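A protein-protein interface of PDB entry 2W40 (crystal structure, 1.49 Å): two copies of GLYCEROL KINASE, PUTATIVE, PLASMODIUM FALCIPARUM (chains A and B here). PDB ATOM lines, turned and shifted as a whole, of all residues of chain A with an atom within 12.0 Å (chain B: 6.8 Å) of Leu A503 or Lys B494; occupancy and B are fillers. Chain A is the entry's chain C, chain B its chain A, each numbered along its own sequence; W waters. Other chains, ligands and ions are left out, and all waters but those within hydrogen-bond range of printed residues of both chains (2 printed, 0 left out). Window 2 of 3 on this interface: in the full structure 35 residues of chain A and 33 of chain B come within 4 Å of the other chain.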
ATOM      1  N   ARG A 361      21.611  43.614   4.450  1.00  0.00           N
ATOM      2  CA  ARG A 361      20.551  42.649   4.173  1.00  0.00           C
ATOM      3  C   ARG A 361      19.913  42.257   5.490  1.00  0.00           C
ATOM      4  O   ARG A 361      20.373  41.371   6.184  1.00  0.00           O
ATOM      5  CB  ARG A 361      21.197  41.471   3.445  1.00  0.00           C
ATOM      6  CG  ARG A 361      21.548  41.793   2.056  1.00  0.00           C
ATOM      7  CD  ARG A 361      20.314  42.001   1.110  1.00  0.00           C
ATOM      8  NE  ARG A 361      19.512  40.770   0.998  1.00  0.00           N
ATOM      9  CZ  ARG A 361      19.657  39.850   0.027  1.00  0.00           C
ATOM     10  NH1 ARG A 361      20.560  39.961  -0.940  1.00  0.00           N
ATOM     11  NH2 ARG A 361      18.909  38.764   0.082  1.00  0.00           N
ATOM     12  N   ASP A 363      17.182  40.717   5.818  1.00  0.00           N
ATOM     13  CA  ASP A 363      16.599  39.362   5.591  1.00  0.00           C
ATOM     14  C   ASP A 363      17.572  38.205   5.852  1.00  0.00           C
ATOM     15  O   ASP A 363      17.163  37.062   5.990  1.00  0.00           O
ATOM     16  CB  ASP A 363      16.016  39.252   4.187  1.00  0.00           C
ATOM     17  CG  ASP A 363      16.996  39.530   3.096  1.00  0.00           C
ATOM     18  OD1 ASP A 363      17.939  40.354   3.204  1.00  0.00           O
ATOM     19  OD2 ASP A 363      16.711  38.976   1.996  1.00  0.00           O
ATOM     20  N   ALA A 364      18.863  38.497   5.975  1.00  0.00           N
ATOM     21  CA  ALA A 364      19.857  37.480   6.354  1.00  0.00           C
ATOM     22  C   ALA A 364      19.576  36.985   7.765  1.00  0.00           C
ATOM     23  O   ALA A 364      19.284  37.762   8.651  1.00  0.00           O
ATOM     24  CB  ALA A 364      21.268  38.044   6.238  1.00  0.00           C
ATOM     25  N   SER A 367      23.621  31.438   9.764  1.00  0.00           N
ATOM     26  CA  SER A 367      23.615  30.173   9.016  1.00  0.00           C
ATOM     27  C   SER A 367      24.960  29.479   9.215  1.00  0.00           C
ATOM     28  O   SER A 367      25.991  30.110   9.251  1.00  0.00           O
ATOM     29  CB  SER A 367      23.472  30.481   7.543  1.00  0.00           C
ATOM     30  OG  SER A 367      22.302  31.297   7.397  1.00  0.00           O
ATOM     31  N   ILE A 368      24.944  28.157   9.379  1.00  0.00           N
ATOM     32  CA  ILE A 368      26.161  27.314   9.498  1.00  0.00           C
ATOM     33  C   ILE A 368      26.168  26.292   8.396  1.00  0.00           C
ATOM     34  O   ILE A 368      25.129  25.643   8.155  1.00  0.00           O
ATOM     35  CB  ILE A 368      26.262  26.588  10.880  1.00  0.00           C
ATOM     36  CG1 ILE A 368      26.147  27.553  12.030  1.00  0.00           C
ATOM     37  CG2 ILE A 368      27.629  25.867  11.023  1.00  0.00           C
ATOM     38  CD1 ILE A 368      26.112  26.995  13.429  1.00  0.00           C
ATOM     39  N   TYR A 369      27.291  26.198   7.674  1.00  0.00           N
ATOM     40  CA  TYR A 369      27.441  25.284   6.569  1.00  0.00           C
ATOM     41  C   TYR A 369      28.631  24.370   6.748  1.00  0.00           C
ATOM     42  O   TYR A 369      29.592  24.708   7.429  1.00  0.00           O
ATOM     43  CB  TYR A 369      27.700  26.072   5.273  1.00  0.00           C
ATOM     44  CG  TYR A 369      26.641  27.057   4.962  1.00  0.00           C
ATOM     45  CD1 TYR A 369      25.512  26.650   4.264  1.00  0.00           C
ATOM     46  CD2 TYR A 369      26.717  28.403   5.361  1.00  0.00           C
ATOM     47  CE1 TYR A 369      24.474  27.550   3.958  1.00  0.00           C
ATOM     48  CE2 TYR A 369      25.672  29.315   4.970  1.00  0.00           C
ATOM     49  CZ  TYR A 369      24.563  28.850   4.362  1.00  0.00           C
ATOM     50  OH  TYR A 369      23.558  29.722   4.032  1.00  0.00           O
ATOM     51  N   LYS A 494      30.594  32.129  -1.233  1.00  0.00           N
ATOM     52  CA  LYS A 494      29.581  31.147  -1.656  1.00  0.00           C
ATOM     53  C   LYS A 494      28.612  30.868  -0.521  1.00  0.00           C
ATOM     54  O   LYS A 494      27.417  30.750  -0.730  1.00  0.00           O
ATOM     55  CB  LYS A 494      30.250  29.888  -2.111  1.00  0.00           C
ATOM     56  CG  LYS A 494      30.986  30.095  -3.389  1.00  0.00           C
ATOM     57  CD  LYS A 494      31.384  28.853  -4.063  1.00  0.00           C
ATOM     58  CE  LYS A 494      31.394  27.581  -3.181  1.00  0.00           C
ATOM     59  NZ  LYS A 494      32.682  27.362  -2.371  1.00  0.00           N
ATOM     60  N   ALA A 495      29.100  30.786   0.730  1.00  0.00           N
ATOM     61  CA  ALA A 495      28.232  30.629   1.925  1.00  0.00           C
ATOM     62  C   ALA A 495      27.351  31.853   2.103  1.00  0.00           C
ATOM     63  O   ALA A 495      26.162  31.723   2.297  1.00  0.00           O
ATOM     64  CB  ALA A 495      29.134  30.489   3.136  1.00  0.00           C
ATOM     65  N   VAL A 496      27.854  33.061   1.899  1.00  0.00           N
ATOM     66  CA  VAL A 496      26.962  34.291   1.918  1.00  0.00           C
ATOM     67  C   VAL A 496      25.902  34.259   0.798  1.00  0.00           C
ATOM     68  O   VAL A 496      24.663  34.471   0.996  1.00  0.00           O
ATOM     69  CB  VAL A 496      27.768  35.574   1.905  1.00  0.00           C
ATOM     70  CG1 VAL A 496      26.836  36.778   1.906  1.00  0.00           C
ATOM     71  CG2 VAL A 496      28.680  35.617   3.135  1.00  0.00           C
ATOM     72  N   GLU A 497      26.317  33.805  -0.351  1.00  0.00           N
ATOM     73  CA  GLU A 497      25.337  33.677  -1.486  1.00  0.00           C
ATOM     74  C   GLU A 497      24.251  32.702  -1.106  1.00  0.00           C
ATOM     75  O   GLU A 497      23.050  32.931  -1.420  1.00  0.00           O
ATOM     76  CB  GLU A 497      26.071  33.262  -2.764  1.00  0.00           C
ATOM     77  CG  GLU A 497      25.225  33.323  -3.962  1.00  0.00           C
ATOM     78  CD  GLU A 497      26.031  33.109  -5.255  1.00  0.00           C
ATOM     79  OE1 GLU A 497      27.293  32.900  -5.161  1.00  0.00           O
ATOM     80  OE2 GLU A 497      25.353  33.134  -6.332  1.00  0.00           O
ATOM     81  N   ARG A 498      24.613  31.528  -0.561  1.00  0.00           N
ATOM     82  CA  ARG A 498      23.637  30.492  -0.107  1.00  0.00           C
ATOM     83  C   ARG A 498      22.680  31.135   0.886  1.00  0.00           C
ATOM     84  O   ARG A 498      21.463  30.845   0.886  1.00  0.00           O
ATOM     85  CB  ARG A 498      24.257  29.247   0.570  1.00  0.00           C
ATOM     86  CG  ARG A 498      25.030  28.385  -0.279  1.00  0.00           C
ATOM     87  CD  ARG A 498      25.495  27.194   0.485  1.00  0.00           C
ATOM     88  NE  ARG A 498      26.602  26.663  -0.281  1.00  0.00           N
ATOM     89  CZ  ARG A 498      26.438  26.068  -1.477  1.00  0.00           C
ATOM     90  NH1 ARG A 498      25.243  25.660  -1.898  1.00  0.00           N
ATOM     91  NH2 ARG A 498      27.510  25.697  -2.175  1.00  0.00           N
ATOM     92  N   THR A 499      23.201  31.955   1.769  1.00  0.00           N
ATOM     93  CA  THR A 499      22.404  32.565   2.843  1.00  0.00           C
ATOM     94  C   THR A 499      21.383  33.634   2.305  1.00  0.00           C
ATOM     95  O   THR A 499      20.330  33.893   2.877  1.00  0.00           O
ATOM     96  CB  THR A 499      23.375  33.229   3.843  1.00  0.00           C
ATOM     97  OG1 THR A 499      24.271  32.217   4.308  1.00  0.00           O
ATOM     98  CG2 THR A 499      22.598  33.919   5.030  1.00  0.00           C
ATOM     99  N   LEU A 500      21.750  34.279   1.219  1.00  0.00           N
ATOM    100  CA  LEU A 500      21.028  35.472   0.659  1.00  0.00           C
ATOM    101  C   LEU A 500      20.157  35.136  -0.550  1.00  0.00           C
ATOM    102  O   LEU A 500      19.301  35.954  -0.912  1.00  0.00           O
ATOM    103  CB  LEU A 500      22.049  36.560   0.300  1.00  0.00           C
ATOM    104  CG  LEU A 500      22.841  37.230   1.445  1.00  0.00           C
ATOM    105  CD1 LEU A 500      23.734  38.314   0.882  1.00  0.00           C
ATOM    106  CD2 LEU A 500      21.935  37.823   2.515  1.00  0.00           C
ATOM    107  N   ILE A 501      20.427  34.049  -1.247  1.00  0.00           N
ATOM    108  CA  ILE A 501      19.712  33.751  -2.498  1.00  0.00           C
ATOM    109  C   ILE A 501      18.191  33.700  -2.257  1.00  0.00           C
ATOM    110  O   ILE A 501      17.691  33.213  -1.237  1.00  0.00           O
ATOM    111  CB  ILE A 501      20.303  32.486  -3.241  1.00  0.00           C
ATOM    112  CG1 ILE A 501      19.780  32.381  -4.677  1.00  0.00           C
ATOM    113  CG2 ILE A 501      20.014  31.297  -2.444  1.00  0.00           C
ATOM    114  CD1 ILE A 501      20.576  31.446  -5.531  1.00  0.00           C
ATOM    115  N   GLN A 502      17.468  34.317  -3.181  1.00  0.00           N
ATOM    116  CA  GLN A 502      16.023  34.392  -3.133  1.00  0.00           C
ATOM    117  C   GLN A 502      15.451  33.201  -3.884  1.00  0.00           C
ATOM    118  O   GLN A 502      15.793  32.962  -5.054  1.00  0.00           O
ATOM    119  CB  GLN A 502      15.548  35.744  -3.740  1.00  0.00           C
ATOM    120  CG  GLN A 502      15.854  36.961  -2.894  1.00  0.00           C
ATOM    121  CD  GLN A 502      15.409  36.764  -1.487  1.00  0.00           C
ATOM    122  OE1 GLN A 502      16.186  36.273  -0.619  1.00  0.00           O
ATOM    123  NE2 GLN A 502      14.130  37.060  -1.231  1.00  0.00           N
ATOM    124  N   LEU A 503      14.664  32.393  -3.151  1.00  0.00           N
ATOM    125  CA  LEU A 503      14.084  31.113  -3.649  1.00  0.00           C
ATOM    126  C   LEU A 503      12.540  31.142  -3.487  1.00  0.00           C
ATOM    127  O   LEU A 503      12.013  31.695  -2.472  1.00  0.00           O
ATOM    128  CB  LEU A 503      14.655  29.944  -2.798  1.00  0.00           C
ATOM    129  CG  LEU A 503      16.160  29.793  -2.872  1.00  0.00           C
ATOM    130  CD1 LEU A 503      16.525  28.759  -1.842  1.00  0.00           C
ATOM    131  CD2 LEU A 503      16.630  29.460  -4.273  1.00  0.00           C
ATOM    132  N   ILE B 347      15.767  25.905  10.240  1.00  0.00           N
ATOM    133  CA  ILE B 347      15.764  24.643   9.555  1.00  0.00           C
ATOM    134  C   ILE B 347      17.192  24.081   9.652  1.00  0.00           C
ATOM    135  O   ILE B 347      18.164  24.779   9.487  1.00  0.00           O
ATOM    136  CB  ILE B 347      15.330  24.750   8.047  1.00  0.00           C
ATOM    137  CG1 ILE B 347      13.953  25.421   7.982  1.00  0.00           C
ATOM    138  CG2 ILE B 347      15.466  23.399   7.296  1.00  0.00           C
ATOM    139  CD1 ILE B 347      13.499  25.857   6.608  1.00  0.00           C
ATOM    140  N   ARG B 359      17.452  11.699  -2.649  1.00  0.00           N
ATOM    141  CA  ARG B 359      18.298  12.588  -3.467  1.00  0.00           C
ATOM    142  C   ARG B 359      19.755  12.135  -3.777  1.00  0.00           C
ATOM    143  O   ARG B 359      20.317  12.463  -4.806  1.00  0.00           O
ATOM    144  CB  ARG B 359      18.303  14.000  -2.900  1.00  0.00           C
ATOM    145  CG  ARG B 359      16.972  14.657  -2.749  1.00  0.00           C
ATOM    146  CD  ARG B 359      17.082  16.109  -2.344  1.00  0.00           C
ATOM    147  NE  ARG B 359      15.823  16.678  -1.852  1.00  0.00           N
ATOM    148  CZ  ARG B 359      15.416  17.907  -2.087  1.00  0.00           C
ATOM    149  NH1 ARG B 359      16.035  18.643  -2.959  1.00  0.00           N
ATOM    150  NH2 ARG B 359      14.286  18.352  -1.541  1.00  0.00           N
ATOM    151  N   TYR B 369      19.966  26.958   9.197  1.00  0.00           N
ATOM    152  CA  TYR B 369      19.495  28.187   8.601  1.00  0.00           C
ATOM    153  C   TYR B 369      18.525  28.866   9.560  1.00  0.00           C
ATOM    154  O   TYR B 369      17.849  28.182  10.374  1.00  0.00           O
ATOM    155  CB  TYR B 369      18.754  27.961   7.272  1.00  0.00           C
ATOM    156  CG  TYR B 369      19.571  27.275   6.272  1.00  0.00           C
ATOM    157  CD1 TYR B 369      20.384  28.005   5.474  1.00  0.00           C
ATOM    158  CD2 TYR B 369      19.493  25.899   6.071  1.00  0.00           C
ATOM    159  CE1 TYR B 369      21.177  27.439   4.498  1.00  0.00           C
ATOM    160  CE2 TYR B 369      20.301  25.273   5.067  1.00  0.00           C
ATOM    161  CZ  TYR B 369      21.149  26.037   4.307  1.00  0.00           C
ATOM    162  OH  TYR B 369      21.935  25.402   3.348  1.00  0.00           O
ATOM    163  N   LYS B 487       3.279  24.716   3.319  1.00  0.00           N
ATOM    164  CA  LYS B 487       4.190  25.763   3.711  1.00  0.00           C
ATOM    165  C   LYS B 487       5.497  25.233   4.279  1.00  0.00           C
ATOM    166  O   LYS B 487       6.614  25.727   3.961  1.00  0.00           O
ATOM    167  CB  LYS B 487       3.518  26.692   4.724  1.00  0.00           C
ATOM    168  CG  LYS B 487       4.366  27.928   5.102  1.00  0.00           C
ATOM    169  CD  LYS B 487       3.830  28.636   6.371  1.00  0.00           C
ATOM    170  CE  LYS B 487       4.423  30.077   6.557  1.00  0.00           C
ATOM    171  NZ  LYS B 487       5.902  30.050   6.652  1.00  0.00           N
ATOM    172  N   THR B 489       6.746  22.235   4.147  1.00  0.00           N
ATOM    173  CA  THR B 489       7.538  21.412   3.235  1.00  0.00           C
ATOM    174  C   THR B 489       8.229  22.327   2.221  1.00  0.00           C
ATOM    175  O   THR B 489       9.393  22.052   1.786  1.00  0.00           O
ATOM    176  CB  THR B 489       6.781  20.221   2.633  1.00  0.00           C
ATOM    177  OG1 THR B 489       5.750  20.699   1.806  1.00  0.00           O
ATOM    178  CG2 THR B 489       6.138  19.284   3.678  1.00  0.00           C
ATOM    179  N   SER B 490       7.560  23.435   1.824  1.00  0.00           N
ATOM    180  CA  SER B 490       8.200  24.442   0.991  1.00  0.00           C
ATOM    181  C   SER B 490       9.456  25.106   1.635  1.00  0.00           C
ATOM    182  O   SER B 490      10.497  25.277   0.914  1.00  0.00           O
ATOM    183  CB  SER B 490       7.183  25.517   0.562  1.00  0.00           C
ATOM    184  OG  SER B 490       7.830  26.268  -0.451  1.00  0.00           O
ATOM    185  N   GLU B 491       9.395  25.420   2.943  1.00  0.00           N
ATOM    186  CA  GLU B 491      10.471  25.955   3.745  1.00  0.00           C
ATOM    187  C   GLU B 491      11.656  24.964   3.845  1.00  0.00           C
ATOM    188  O   GLU B 491      12.843  25.303   3.671  1.00  0.00           O
ATOM    189  CB  GLU B 491      10.048  26.234   5.174  1.00  0.00           C
ATOM    190  CG  GLU B 491       9.155  27.475   5.342  1.00  0.00           C
ATOM    191  CD  GLU B 491       8.286  27.507   6.565  1.00  0.00           C
ATOM    192  OE1 GLU B 491       8.265  26.585   7.412  1.00  0.00           O
ATOM    193  OE2 GLU B 491       7.518  28.537   6.606  1.00  0.00           O
ATOM    194  N   TRP B 492      11.303  23.689   4.062  1.00  0.00           N
ATOM    195  CA  TRP B 492      12.369  22.621   4.037  1.00  0.00           C
ATOM    196  C   TRP B 492      13.012  22.545   2.637  1.00  0.00           C
ATOM    197  O   TRP B 492      14.248  22.543   2.490  1.00  0.00           O
ATOM    198  CB  TRP B 492      11.737  21.267   4.426  1.00  0.00           C
ATOM    199  CG  TRP B 492      12.549  20.099   4.082  1.00  0.00           C
ATOM    200  CD1 TRP B 492      12.414  19.276   3.001  1.00  0.00           C
ATOM    201  CD2 TRP B 492      13.700  19.582   4.840  1.00  0.00           C
ATOM    202  NE1 TRP B 492      13.410  18.308   3.019  1.00  0.00           N
ATOM    203  CE2 TRP B 492      14.199  18.480   4.116  1.00  0.00           C
ATOM    204  CE3 TRP B 492      14.346  19.959   6.028  1.00  0.00           C
ATOM    205  CZ2 TRP B 492      15.307  17.739   4.532  1.00  0.00           C
ATOM    206  CZ3 TRP B 492      15.424  19.173   6.462  1.00  0.00           C
ATOM    207  CH2 TRP B 492      15.908  18.103   5.686  1.00  0.00           C
ATOM    208  N   ASN B 493      12.207  22.561   1.592  1.00  0.00           N
ATOM    209  CA  ASN B 493      12.691  22.376   0.232  1.00  0.00           C
ATOM    210  C   ASN B 493      13.650  23.512  -0.161  1.00  0.00           C
ATOM    211  O   ASN B 493      14.663  23.274  -0.840  1.00  0.00           O
ATOM    212  CB  ASN B 493      11.513  22.375  -0.801  1.00  0.00           C
ATOM    213  CG  ASN B 493      10.782  21.085  -0.861  1.00  0.00           C
ATOM    214  OD1 ASN B 493      11.230  20.055  -0.365  1.00  0.00           O
ATOM    215  ND2 ASN B 493       9.602  21.112  -1.528  1.00  0.00           N
ATOM    216  N   LYS B 494      13.340  24.736   0.257  1.00  0.00           N
ATOM    217  CA  LYS B 494      14.232  25.863   0.011  1.00  0.00           C
ATOM    218  C   LYS B 494      15.532  25.746   0.762  1.00  0.00           C
ATOM    219  O   LYS B 494      16.584  26.071   0.176  1.00  0.00           O
ATOM    220  CB  LYS B 494      13.595  27.173   0.410  1.00  0.00           C
ATOM    221  CG  LYS B 494      12.493  27.548  -0.582  1.00  0.00           C
ATOM    222  CD  LYS B 494      11.855  28.880  -0.066  1.00  0.00           C
ATOM    223  CE  LYS B 494      10.748  29.407  -0.980  1.00  0.00           C
ATOM    224  NZ  LYS B 494       9.666  28.399  -1.194  1.00  0.00           N
ATOM    225  N   ALA B 495      15.477  25.299   2.040  1.00  0.00           N
ATOM    226  CA  ALA B 495      16.675  25.039   2.780  1.00  0.00           C
ATOM    227  C   ALA B 495      17.556  23.999   2.111  1.00  0.00           C
ATOM    228  O   ALA B 495      18.796  24.150   2.053  1.00  0.00           O
ATOM    229  CB  ALA B 495      16.372  24.559   4.165  1.00  0.00           C
ATOM    230  N   VAL B 496      16.956  22.923   1.640  1.00  0.00           N
ATOM    231  CA  VAL B 496      17.722  21.862   0.991  1.00  0.00           C
ATOM    232  C   VAL B 496      18.315  22.433  -0.280  1.00  0.00           C
ATOM    233  O   VAL B 496      19.491  22.175  -0.614  1.00  0.00           O
ATOM    234  CB  VAL B 496      16.889  20.604   0.690  1.00  0.00           C
ATOM    235  CG1 VAL B 496      17.735  19.628  -0.198  1.00  0.00           C
ATOM    236  CG2 VAL B 496      16.385  20.007   2.001  1.00  0.00           C
ATOM    237  N   GLU B 497      17.545  23.194  -1.034  1.00  0.00           N
ATOM    238  CA  GLU B 497      18.063  23.822  -2.248  1.00  0.00           C
ATOM    239  C   GLU B 497      19.280  24.726  -1.952  1.00  0.00           C
ATOM    240  O   GLU B 497      20.300  24.666  -2.696  1.00  0.00           O
ATOM    241  CB  GLU B 497      16.938  24.648  -2.946  1.00  0.00           C
ATOM    242  CG  GLU B 497      17.322  25.213  -4.287  1.00  0.00           C
ATOM    243  CD  GLU B 497      16.128  25.778  -5.078  1.00  0.00           C
ATOM    244  OE1 GLU B 497      16.411  26.107  -6.276  1.00  0.00           O
ATOM    245  OE2 GLU B 497      14.957  25.899  -4.513  1.00  0.00           O
ATOM    246  N   ARG B 498      19.226  25.551  -0.904  1.00  0.00           N
ATOM    247  CA  ARG B 498      20.388  26.355  -0.427  1.00  0.00           C
ATOM    248  C   ARG B 498      21.586  25.464  -0.120  1.00  0.00           C
ATOM    249  O   ARG B 498      22.746  25.800  -0.389  1.00  0.00           O
ATOM    250  CB  ARG B 498      20.159  27.167   0.874  1.00  0.00           C
ATOM    251  CG  ARG B 498      19.271  28.333   0.809  1.00  0.00           C
ATOM    252  CD  ARG B 498      19.057  28.974   2.147  1.00  0.00           C
ATOM    253  NE  ARG B 498      17.800  29.716   1.922  1.00  0.00           N
ATOM    254  CZ  ARG B 498      17.687  30.805   1.138  1.00  0.00           C
ATOM    255  NH1 ARG B 498      18.733  31.410   0.532  1.00  0.00           N
ATOM    256  NH2 ARG B 498      16.491  31.315   0.959  1.00  0.00           N
ATOM    257  N   THR B 499      21.324  24.306   0.466  1.00  0.00           N
ATOM    258  CA  THR B 499      22.375  23.359   0.833  1.00  0.00           C
ATOM    259  C   THR B 499      23.047  22.721  -0.391  1.00  0.00           C
ATOM    260  O   THR B 499      24.271  22.351  -0.345  1.00  0.00           O
ATOM    261  CB  THR B 499      21.784  22.301   1.767  1.00  0.00           C
ATOM    262  OG1 THR B 499      21.240  22.944   2.926  1.00  0.00           O
ATOM    263  CG2 THR B 499      22.819  21.203   2.253  1.00  0.00           C
ATOM    264  N   ILE B 501      22.780  23.878  -3.916  1.00  0.00           N
ATOM    265  CA  ILE B 501      23.003  24.690  -5.110  1.00  0.00           C
ATOM    266  C   ILE B 501      24.521  24.646  -5.384  1.00  0.00           C
ATOM    267  O   ILE B 501      25.375  24.791  -4.463  1.00  0.00           O
ATOM    268  CB  ILE B 501      22.375  26.150  -4.998  1.00  0.00           C
ATOM    269  CG1 ILE B 501      22.362  26.871  -6.384  1.00  0.00           C
ATOM    270  CG2 ILE B 501      23.001  26.878  -3.914  1.00  0.00           C
ATOM    271  CD1 ILE B 501      21.335  27.997  -6.478  1.00  0.00           C
HETATM  272  O   HOH W   1      14.232  32.952  -0.350  1.00  0.00           O
HETATM  273  O   HOH W   2      28.839  24.828  -4.857  1.00  0.00           O
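Of the 16 printed residues of chain A, 5 touch a printed residue of chain B.
Hydrophobic or aromatic side chains of chain A within 4 Å of the printed part of chain B: Tyr A369, Ile A501 and Leu A503.
Hydrophobic or aromatic side chains of chain B that line the printed part of chain A: Tyr B369 and Ile B501.
Among the printed residues, 10 pairs touch across the chains.
Among the printed residues, no Asp or Glu carboxylate lies within 4 Å of a Lys or Arg side-chain nitrogen of the other chain.
Leu A503 touches just these residues of chain B: Lys B494 (3.0 Å), Glu B497 (3.8 Å) and Arg B498 (3.8 Å).
Lys B494 touches one residue of chain A.
No residue of chain A comes within 4 Å of Ser B490.
No residue of chain A comes within 4 Å of Asn B493.
No residue of chain A comes within 4 Å of Ala B495.
Val B496 touches none of the printed residues of chain A.
Of chain A, only Arg A498, Thr A499, Ile A501 and Leu A503 come within 4 Å of Arg B498.
Printed residues of chain A within 4 Å of Tyr B369: Tyr A369 (3.3 Å).
Printed residues of chain B within 4 Å of Arg A498: Arg B498, Thr B499 and Ile B501.
Printed residues of chain A within 4 Å of Thr B499: Arg A498.
Printed residues of chain B within 4 Å of Tyr A369: Tyr B369 (3.3 Å).
Of the printed residues of chain B, Thr A499 touches Arg B498.
Lys A494 touches none of the printed residues of chain B.
The nearest residue of chain B that does not touch Leu A503 is Ala B495 (5.3 Å).
Water W1 bridges the backbone NH of Leu A503 (2.9 Å) and the guanidinium group of Arg B498 (3.1 Å).
Water W2 lies within hydrogen-bond range of the guanidinium group (NH2) of Arg A498 (3.1 Å) and the backbone carbonyl oxygen (O) of Ile B501 (3.5 Å).
O of Ile A501 sits at hydrogen-bond distance from NH1 of Arg B498 (2.7 Å).
The backbone carbonyl oxygen (O) of Ile B501 lies within hydrogen-bond range of the guanidinium group (NH1) of Arg A498, 2.7 Å away.
The backbone carbonyl oxygen (O) of Arg A498 is in hydrogen-bond range of the guanidinium group (NH1) of Arg B498 (2.8 Å).
Tyr A369 touches its own counterpart, Tyr B369.
Arg A498 touches Thr B499, and with the chains exchanged Thr A499 touches Arg B498.
Arg A498 touches Ile B501, and with the chains exchanged Ile A501 touches Arg B498.
Ile B501 touches its own counterpart, Ile A501.
8 positions are printed for both chains.
OG1 of Thr B499 lies within hydrogen-bond range of O of Ala B495 (2.9 Å).
OG of Ser B490 lies within hydrogen-bond range of NZ of Lys B494 (2.9 Å).
The backbone carbonyl oxygen (O) of Ile B347 is in hydrogen-bond range of the backbone NH (N) of Tyr B369 (2.8 Å).
The side-chain hydroxyl (OH) of Tyr A369 sits at hydrogen-bond distance from the side-chain hydroxyl (OG1) of Thr A499.
The side-chain hydroxyl (OG1) of Thr B499 sits at hydrogen-bond distance from the side-chain hydroxyl (OH) of Tyr B369, at 2.6 Å.
O of Ala A495 lies within hydrogen-bond range of OG1 of Thr A499.
Among the printed residues, pairs that only touch across the chains: Leu A503 with Lys B494 (3.0 Å), Tyr A369 with Tyr B369 (3.3 Å), Ile A501 with Ile B501 (3.7 Å), Thr A499 with Arg B498 (3.8 Å), Arg A498 with Thr B499 (3.8 Å), Leu A503 with Arg B498 (3.8 Å) and Leu A503 with Glu B497 (3.8 Å).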
